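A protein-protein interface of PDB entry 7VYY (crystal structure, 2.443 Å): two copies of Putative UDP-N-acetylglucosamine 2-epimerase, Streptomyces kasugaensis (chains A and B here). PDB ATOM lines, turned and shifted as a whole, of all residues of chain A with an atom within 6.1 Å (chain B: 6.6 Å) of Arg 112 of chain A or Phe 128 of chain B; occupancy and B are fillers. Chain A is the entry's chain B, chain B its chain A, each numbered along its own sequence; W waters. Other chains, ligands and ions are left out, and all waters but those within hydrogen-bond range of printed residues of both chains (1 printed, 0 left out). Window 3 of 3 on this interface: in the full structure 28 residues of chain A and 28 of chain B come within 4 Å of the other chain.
NH2 of Arg 127 of chain B lies within hydrogen-bond range of O of Gln 142 of chain A (3.2 Å). The backbone carbonyl oxygen of Gln 142 of chain A lies within hydrogen-bond range of the guanidinium group of Arg 138 of chain B, at 2.8 Å. NH2 of Arg 127 of chain B is in salt-bridge range of OD1 of Asp 145 of chain A, 3.5 Å away. The guanidinium group of Arg 127 of chain B lies within hydrogen-bond range of the backbone carbonyl oxygen of Leu 143 of chain A, 3.4 Å away.
The side-chain carboxylate (OE1) of Glu 134 of chain B lies within salt-bridge range of the guanidinium group (NH2) of Arg 138 of chain B (2.8 Å). OE1 of Glu 134 of chain B sits at hydrogen-bond distance from N of Phe 128 of chain B.
Among the printed residues, merely in contact across the chains: Ala 109 of chain A with Phe 131 of chain B (3.1 Å), Cys 110 of chain A with Phe 131 of chain B (3.8 Å), Arg 112 of chain A with Phe 128 of chain B (3.6 Å), Arg 112 of chain A with Phe 131 of chain B (3.4 Å), Gln 142 of chain A with Ile 135 of chain B (3.2 Å), Leu 143 of chain A with Ile 135 of chain B (3.6 Å) and Asp 145 of chain A with Phe 128 of chain B (3.6 Å).
Arg 112 of chain A touches just these residues of chain B: Phe 128 (3.6 Å) and Phe 131 (3.4 Å). Ile 113 of chain A touches none of the printed residues of chain B. Printed residues of chain B within 4 Å of Leu 143 of chain A: Arg 127 and Ile 135. Printed residues of chain A within 4 Å of Arg 127 of chain B: Gln 142 (3.2 Å), Leu 143 (3.4 Å) and Asp 145 (3.5 Å). Of chain A, only Arg 112 (3.6 Å) and Asp 145 (3.6 Å) come within 4 Å of Phe 128 of chain B. Printed residues of chain A within 4 Å of Phe 131 of chain B: Ala 109 (3.1 Å), Cys 110 (3.8 Å) and Arg 112 (3.4 Å). Glu 134 of chain B touches none of the printed residues of chain A. Of the printed residues of chain A, Arg 138 of chain B touches Gln 142 (2.8 Å). The nearest residue of chain B that does not touch Arg 112 of chain A is Glu 129 of chain B (5.8 Å). The nearest residue of chain A that does not touch Phe 128 of chain B is Leu 143 of chain A (4.1 Å).
Hydrophobic or aromatic side chains of chain A that line the printed part of chain B: Leu 143. Along chain A the printed residues that touch a printed residue of chain B span positions 109 to 145. Of the 10 printed residues of chain B, 5 touch a printed residue of chain A. Hydrophobic or aromatic side chains of chain B within 4 Å of the printed part of chain A: Phe 128, Phe 131 and Ile 135. Among the printed residues, 11 pairs touch across the chains.
No position is printed for both chains. Of the 11 pairs that touch across the chains among the printed residues, none has its exchanged pair printed and touching as well.
Water W1 bridges the guanidinium group (NH1) of Arg 127 of chain B and the backbone carbonyl oxygen (O) of Gln 142 of chain A.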
ATOM      1  N   ASP A  90     -17.924  16.495  12.315  1.00  0.00           N
ATOM      2  CA  ASP A  90     -17.975  17.949  11.999  1.00  0.00           C
ATOM      3  C   ASP A  90     -18.147  18.734  13.302  1.00  0.00           C
ATOM      4  O   ASP A  90     -17.499  19.781  13.444  1.00  0.00           O
ATOM      5  CB  ASP A  90     -19.109  18.262  11.020  1.00  0.00           C
ATOM      6  CG  ASP A  90     -18.976  17.536   9.692  1.00  0.00           C
ATOM      7  OD1 ASP A  90     -17.990  17.809   8.999  1.00  0.00           O
ATOM      8  OD2 ASP A  90     -19.862  16.697   9.371  1.00  0.00           O
ATOM      9  N   ALA A 107     -10.231  17.665  23.628  1.00  0.00           N
ATOM     10  CA  ALA A 107      -9.731  16.747  22.576  1.00  0.00           C
ATOM     11  C   ALA A 107     -10.272  17.182  21.208  1.00  0.00           C
ATOM     12  O   ALA A 107      -9.468  17.322  20.258  1.00  0.00           O
ATOM     13  CB  ALA A 107     -10.128  15.330  22.897  1.00  0.00           C
ATOM     14  N   ALA A 108     -11.583  17.421  21.130  1.00  0.00           N
ATOM     15  CA  ALA A 108     -12.272  17.955  19.933  1.00  0.00           C
ATOM     16  C   ALA A 108     -11.642  19.288  19.513  1.00  0.00           C
ATOM     17  O   ALA A 108     -11.407  19.470  18.306  1.00  0.00           O
ATOM     18  CB  ALA A 108     -13.755  18.108  20.202  1.00  0.00           C
ATOM     19  N   ALA A 109     -11.391  20.199  20.461  1.00  0.00           N
ATOM     20  CA  ALA A 109     -10.887  21.564  20.166  1.00  0.00           C
ATOM     21  C   ALA A 109      -9.457  21.488  19.620  1.00  0.00           C
ATOM     22  O   ALA A 109      -9.115  22.326  18.772  1.00  0.00           O
ATOM     23  CB  ALA A 109     -10.974  22.459  21.378  1.00  0.00           C
ATOM     24  N   CYS A 110      -8.662  20.516  20.070  1.00  0.00           N
ATOM     25  CA  CYS A 110      -7.268  20.295  19.587  1.00  0.00           C
ATOM     26  C   CYS A 110      -7.262  19.979  18.084  1.00  0.00           C
ATOM     27  O   CYS A 110      -6.302  20.413  17.397  1.00  0.00           O
ATOM     28  CB  CYS A 110      -6.575  19.175  20.356  1.00  0.00           C
ATOM     29  SG  CYS A 110      -6.180  19.632  22.064  1.00  0.00           S
ATOM     30  N   GLU A 111      -8.295  19.277  17.594  1.00  0.00           N
ATOM     31  CA  GLU A 111      -8.451  18.888  16.163  1.00  0.00           C
ATOM     32  C   GLU A 111      -9.320  19.920  15.429  1.00  0.00           C
ATOM     33  O   GLU A 111      -9.709  19.644  14.273  1.00  0.00           O
ATOM     34  CB  GLU A 111      -9.045  17.484  16.050  1.00  0.00           C
ATOM     35  CG  GLU A 111      -8.319  16.435  16.882  1.00  0.00           C
ATOM     36  CD  GLU A 111      -6.804  16.371  16.736  1.00  0.00           C
ATOM     37  OE1 GLU A 111      -6.287  16.764  15.668  1.00  0.00           O
ATOM     38  OE2 GLU A 111      -6.137  15.913  17.690  1.00  0.00           O
ATOM     39  N   ARG A 112      -9.587  21.065  16.070  1.00  0.00           N
ATOM     40  CA  ARG A 112     -10.345  22.224  15.517  1.00  0.00           C
ATOM     41  C   ARG A 112     -11.790  21.810  15.206  1.00  0.00           C
ATOM     42  O   ARG A 112     -12.391  22.430  14.323  1.00  0.00           O
ATOM     43  CB  ARG A 112      -9.644  22.796  14.275  1.00  0.00           C
ATOM     44  CG  ARG A 112      -8.170  23.147  14.460  1.00  0.00           C
ATOM     45  CD  ARG A 112      -7.901  24.278  15.433  1.00  0.00           C
ATOM     46  NE  ARG A 112      -7.953  25.610  14.830  1.00  0.00           N
ATOM     47  CZ  ARG A 112      -8.857  26.554  15.102  1.00  0.00           C
ATOM     48  NH1 ARG A 112      -9.837  26.341  15.968  1.00  0.00           N
ATOM     49  NH2 ARG A 112      -8.772  27.730  14.504  1.00  0.00           N
ATOM     50  N   ILE A 113     -12.336  20.820  15.920  1.00  0.00           N
ATOM     51  CA  ILE A 113     -13.755  20.372  15.801  1.00  0.00           C
ATOM     52  C   ILE A 113     -14.608  21.203  16.755  1.00  0.00           C
ATOM     53  O   ILE A 113     -14.387  21.193  17.960  1.00  0.00           O
ATOM     54  CB  ILE A 113     -13.886  18.867  16.104  1.00  0.00           C
ATOM     55  CG1 ILE A 113     -13.021  18.017  15.175  1.00  0.00           C
ATOM     56  CG2 ILE A 113     -15.341  18.442  16.070  1.00  0.00           C
ATOM     57  CD1 ILE A 113     -13.138  16.537  15.412  1.00  0.00           C
ATOM     58  N   PRO A 114     -15.613  21.956  16.261  1.00  0.00           N
ATOM     59  CA  PRO A 114     -16.504  22.709  17.144  1.00  0.00           C
ATOM     60  C   PRO A 114     -17.242  21.809  18.151  1.00  0.00           C
ATOM     61  O   PRO A 114     -17.585  20.692  17.801  1.00  0.00           O
ATOM     62  CB  PRO A 114     -17.515  23.378  16.203  1.00  0.00           C
ATOM     63  CG  PRO A 114     -16.880  23.329  14.821  1.00  0.00           C
ATOM     64  CD  PRO A 114     -15.922  22.153  14.837  1.00  0.00           C
ATOM     65  N   GLN A 142     -16.004  27.468  28.229  1.00  0.00           N
ATOM     66  CA  GLN A 142     -14.984  28.233  27.458  1.00  0.00           C
ATOM     67  C   GLN A 142     -14.680  27.506  26.140  1.00  0.00           C
ATOM     68  O   GLN A 142     -14.314  28.205  25.170  1.00  0.00           O
ATOM     69  CB  GLN A 142     -13.716  28.465  28.278  1.00  0.00           C
ATOM     70  CG  GLN A 142     -13.911  29.428  29.441  1.00  0.00           C
ATOM     71  CD  GLN A 142     -14.599  30.711  29.043  1.00  0.00           C
ATOM     72  OE1 GLN A 142     -14.306  31.292  28.001  1.00  0.00           O
ATOM     73  NE2 GLN A 142     -15.510  31.180  29.884  1.00  0.00           N
ATOM     74  N   LEU A 143     -14.843  26.179  26.097  1.00  0.00           N
ATOM     75  CA  LEU A 143     -14.446  25.355  24.926  1.00  0.00           C
ATOM     76  C   LEU A 143     -15.571  25.302  23.889  1.00  0.00           C
ATOM     77  O   LEU A 143     -15.254  25.198  22.693  1.00  0.00           O
ATOM     78  CB  LEU A 143     -14.074  23.946  25.396  1.00  0.00           C
ATOM     79  CG  LEU A 143     -12.685  23.821  26.012  1.00  0.00           C
ATOM     80  CD1 LEU A 143     -12.523  22.479  26.698  1.00  0.00           C
ATOM     81  CD2 LEU A 143     -11.606  24.009  24.956  1.00  0.00           C
ATOM     82  N   ASP A 145     -18.657  26.051  21.344  1.00  0.00           N
ATOM     83  CA  ASP A 145     -19.094  27.080  20.358  1.00  0.00           C
ATOM     84  C   ASP A 145     -20.603  27.302  20.537  1.00  0.00           C
ATOM     85  O   ASP A 145     -21.046  28.458  20.450  1.00  0.00           O
ATOM     86  CB  ASP A 145     -18.755  26.679  18.918  1.00  0.00           C
ATOM     87  CG  ASP A 145     -17.300  26.878  18.512  1.00  0.00           C
ATOM     88  OD1 ASP A 145     -16.404  26.645  19.358  1.00  0.00           O
ATOM     89  OD2 ASP A 145     -17.066  27.244  17.333  1.00  0.00           O
ATOM     90  N   ASP B 126     -10.811  37.738  19.632  1.00  0.00           N
ATOM     91  CA  ASP B 126     -10.854  37.014  18.332  1.00  0.00           C
ATOM     92  C   ASP B 126     -10.716  35.511  18.607  1.00  0.00           C
ATOM     93  O   ASP B 126      -9.572  35.018  18.622  1.00  0.00           O
ATOM     94  CB  ASP B 126      -9.774  37.551  17.385  1.00  0.00           C
ATOM     95  CG  ASP B 126      -9.912  37.123  15.930  1.00  0.00           C
ATOM     96  OD1 ASP B 126     -10.920  36.465  15.588  1.00  0.00           O
ATOM     97  OD2 ASP B 126      -9.007  37.461  15.143  1.00  0.00           O
ATOM     98  N   ARG B 127     -11.852  34.829  18.799  1.00  0.00           N
ATOM     99  CA  ARG B 127     -11.959  33.392  19.181  1.00  0.00           C
ATOM    100  C   ARG B 127     -11.037  32.535  18.300  1.00  0.00           C
ATOM    101  O   ARG B 127     -11.067  32.698  17.065  1.00  0.00           O
ATOM    102  CB  ARG B 127     -13.416  32.924  19.071  1.00  0.00           C
ATOM    103  CG  ARG B 127     -13.665  31.528  19.624  1.00  0.00           C
ATOM    104  CD  ARG B 127     -15.121  31.115  19.667  1.00  0.00           C
ATOM    105  NE  ARG B 127     -15.306  29.858  20.390  1.00  0.00           N
ATOM    106  CZ  ARG B 127     -15.426  29.732  21.716  1.00  0.00           C
ATOM    107  NH1 ARG B 127     -15.357  30.789  22.508  1.00  0.00           N
ATOM    108  NH2 ARG B 127     -15.591  28.534  22.248  1.00  0.00           N
ATOM    109  N   PHE B 128     -10.239  31.669  18.937  1.00  0.00           N
ATOM    110  CA  PHE B 128      -9.346  30.662  18.304  1.00  0.00           C
ATOM    111  C   PHE B 128      -8.383  31.333  17.317  1.00  0.00           C
ATOM    112  O   PHE B 128      -7.976  30.690  16.329  1.00  0.00           O
ATOM    113  CB  PHE B 128     -10.181  29.567  17.637  1.00  0.00           C
ATOM    114  CG  PHE B 128     -10.977  28.684  18.569  1.00  0.00           C
ATOM    115  CD1 PHE B 128     -10.527  28.349  19.843  1.00  0.00           C
ATOM    116  CD2 PHE B 128     -12.177  28.135  18.138  1.00  0.00           C
ATOM    117  CE1 PHE B 128     -11.271  27.514  20.665  1.00  0.00           C
ATOM    118  CE2 PHE B 128     -12.913  27.289  18.957  1.00  0.00           C
ATOM    119  CZ  PHE B 128     -12.465  26.989  20.224  1.00  0.00           C
ATOM    120  N   GLU B 129      -8.017  32.587  17.590  1.00  0.00           N
ATOM    121  CA  GLU B 129      -6.996  33.347  16.829  1.00  0.00           C
ATOM    122  C   GLU B 129      -6.172  34.170  17.819  1.00  0.00           C
ATOM    123  O   GLU B 129      -6.658  35.172  18.348  1.00  0.00           O
ATOM    124  CB  GLU B 129      -7.664  34.212  15.760  1.00  0.00           C
ATOM    125  CG  GLU B 129      -6.686  34.767  14.735  1.00  0.00           C
ATOM    126  CD  GLU B 129      -5.576  33.832  14.274  1.00  0.00           C
ATOM    127  OE1 GLU B 129      -4.409  34.268  14.296  1.00  0.00           O
ATOM    128  OE2 GLU B 129      -5.877  32.678  13.879  1.00  0.00           O
ATOM    129  N   PRO B 130      -4.914  33.770  18.128  1.00  0.00           N
ATOM    130  CA  PRO B 130      -4.310  32.552  17.590  1.00  0.00           C
ATOM    131  C   PRO B 130      -4.770  31.274  18.308  1.00  0.00           C
ATOM    132  O   PRO B 130      -5.335  31.377  19.379  1.00  0.00           O
ATOM    133  CB  PRO B 130      -2.802  32.770  17.781  1.00  0.00           C
ATOM    134  CG  PRO B 130      -2.678  33.763  18.918  1.00  0.00           C
ATOM    135  CD  PRO B 130      -3.991  34.514  18.993  1.00  0.00           C
ATOM    136  N   PHE B 131      -4.512  30.115  17.694  1.00  0.00           N
ATOM    137  CA  PHE B 131      -4.854  28.769  18.221  1.00  0.00           C
ATOM    138  C   PHE B 131      -3.578  28.018  18.591  1.00  0.00           C
ATOM    139  O   PHE B 131      -2.671  27.924  17.768  1.00  0.00           O
ATOM    140  CB  PHE B 131      -5.652  27.954  17.199  1.00  0.00           C
ATOM    141  CG  PHE B 131      -5.993  26.569  17.684  1.00  0.00           C
ATOM    142  CD1 PHE B 131      -7.077  26.359  18.525  1.00  0.00           C
ATOM    143  CD2 PHE B 131      -5.189  25.489  17.361  1.00  0.00           C
ATOM    144  CE1 PHE B 131      -7.366  25.093  19.011  1.00  0.00           C
ATOM    145  CE2 PHE B 131      -5.481  24.224  17.843  1.00  0.00           C
ATOM    146  CZ  PHE B 131      -6.565  24.029  18.669  1.00  0.00           C
ATOM    147  N   PRO B 132      -3.459  27.430  19.811  1.00  0.00           N
ATOM    148  CA  PRO B 132      -4.517  27.435  20.826  1.00  0.00           C
ATOM    149  C   PRO B 132      -4.397  28.516  21.911  1.00  0.00           C
ATOM    150  O   PRO B 132      -5.064  28.389  22.919  1.00  0.00           O
ATOM    151  CB  PRO B 132      -4.298  26.057  21.459  1.00  0.00           C
ATOM    152  CG  PRO B 132      -2.780  25.923  21.487  1.00  0.00           C
ATOM    153  CD  PRO B 132      -2.279  26.683  20.271  1.00  0.00           C
ATOM    154  N   GLU B 134      -5.489  31.495  22.467  1.00  0.00           N
ATOM    155  CA  GLU B 134      -6.670  32.306  22.858  1.00  0.00           C
ATOM    156  C   GLU B 134      -7.577  31.496  23.794  1.00  0.00           C
ATOM    157  O   GLU B 134      -8.084  32.077  24.749  1.00  0.00           O
ATOM    158  CB  GLU B 134      -7.408  32.767  21.597  1.00  0.00           C
ATOM    159  CG  GLU B 134      -8.428  33.858  21.851  1.00  0.00           C
ATOM    160  CD  GLU B 134      -9.821  33.366  22.204  1.00  0.00           C
ATOM    161  OE1 GLU B 134     -10.134  32.196  21.866  1.00  0.00           O
ATOM    162  OE2 GLU B 134     -10.586  34.153  22.829  1.00  0.00           O
ATOM    163  N   ILE B 135      -7.784  30.207  23.513  1.00  0.00           N
ATOM    164  CA  ILE B 135      -8.631  29.303  24.344  1.00  0.00           C
ATOM    165  C   ILE B 135      -7.864  28.959  25.626  1.00  0.00           C
ATOM    166  O   ILE B 135      -8.505  28.916  26.680  1.00  0.00           O
ATOM    167  CB  ILE B 135      -9.092  28.048  23.568  1.00  0.00           C
ATOM    168  CG1 ILE B 135      -9.899  27.087  24.445  1.00  0.00           C
ATOM    169  CG2 ILE B 135      -7.933  27.318  22.921  1.00  0.00           C
ATOM    170  CD1 ILE B 135     -11.115  27.714  25.124  1.00  0.00           C
ATOM    171  N   ARG B 138      -8.331  31.470  28.341  1.00  0.00           N
ATOM    172  CA  ARG B 138      -9.691  31.439  28.931  1.00  0.00           C
ATOM    173  C   ARG B 138      -9.813  30.207  29.835  1.00  0.00           C
ATOM    174  O   ARG B 138     -10.462  30.313  30.888  1.00  0.00           O
ATOM    175  CB  ARG B 138     -10.741  31.540  27.817  1.00  0.00           C
ATOM    176  CG  ARG B 138     -10.814  32.940  27.217  1.00  0.00           C
ATOM    177  CD  ARG B 138     -12.012  33.208  26.326  1.00  0.00           C
ATOM    178  NE  ARG B 138     -11.834  32.572  25.032  1.00  0.00           N
ATOM    179  CZ  ARG B 138     -12.437  31.463  24.616  1.00  0.00           C
ATOM    180  NH1 ARG B 138     -13.299  30.819  25.382  1.00  0.00           N
ATOM    181  NH2 ARG B 138     -12.146  30.984  23.422  1.00  0.00           N
HETATM  182  O   HOH W   1     -17.049  29.814  24.727  1.00  0.00           O
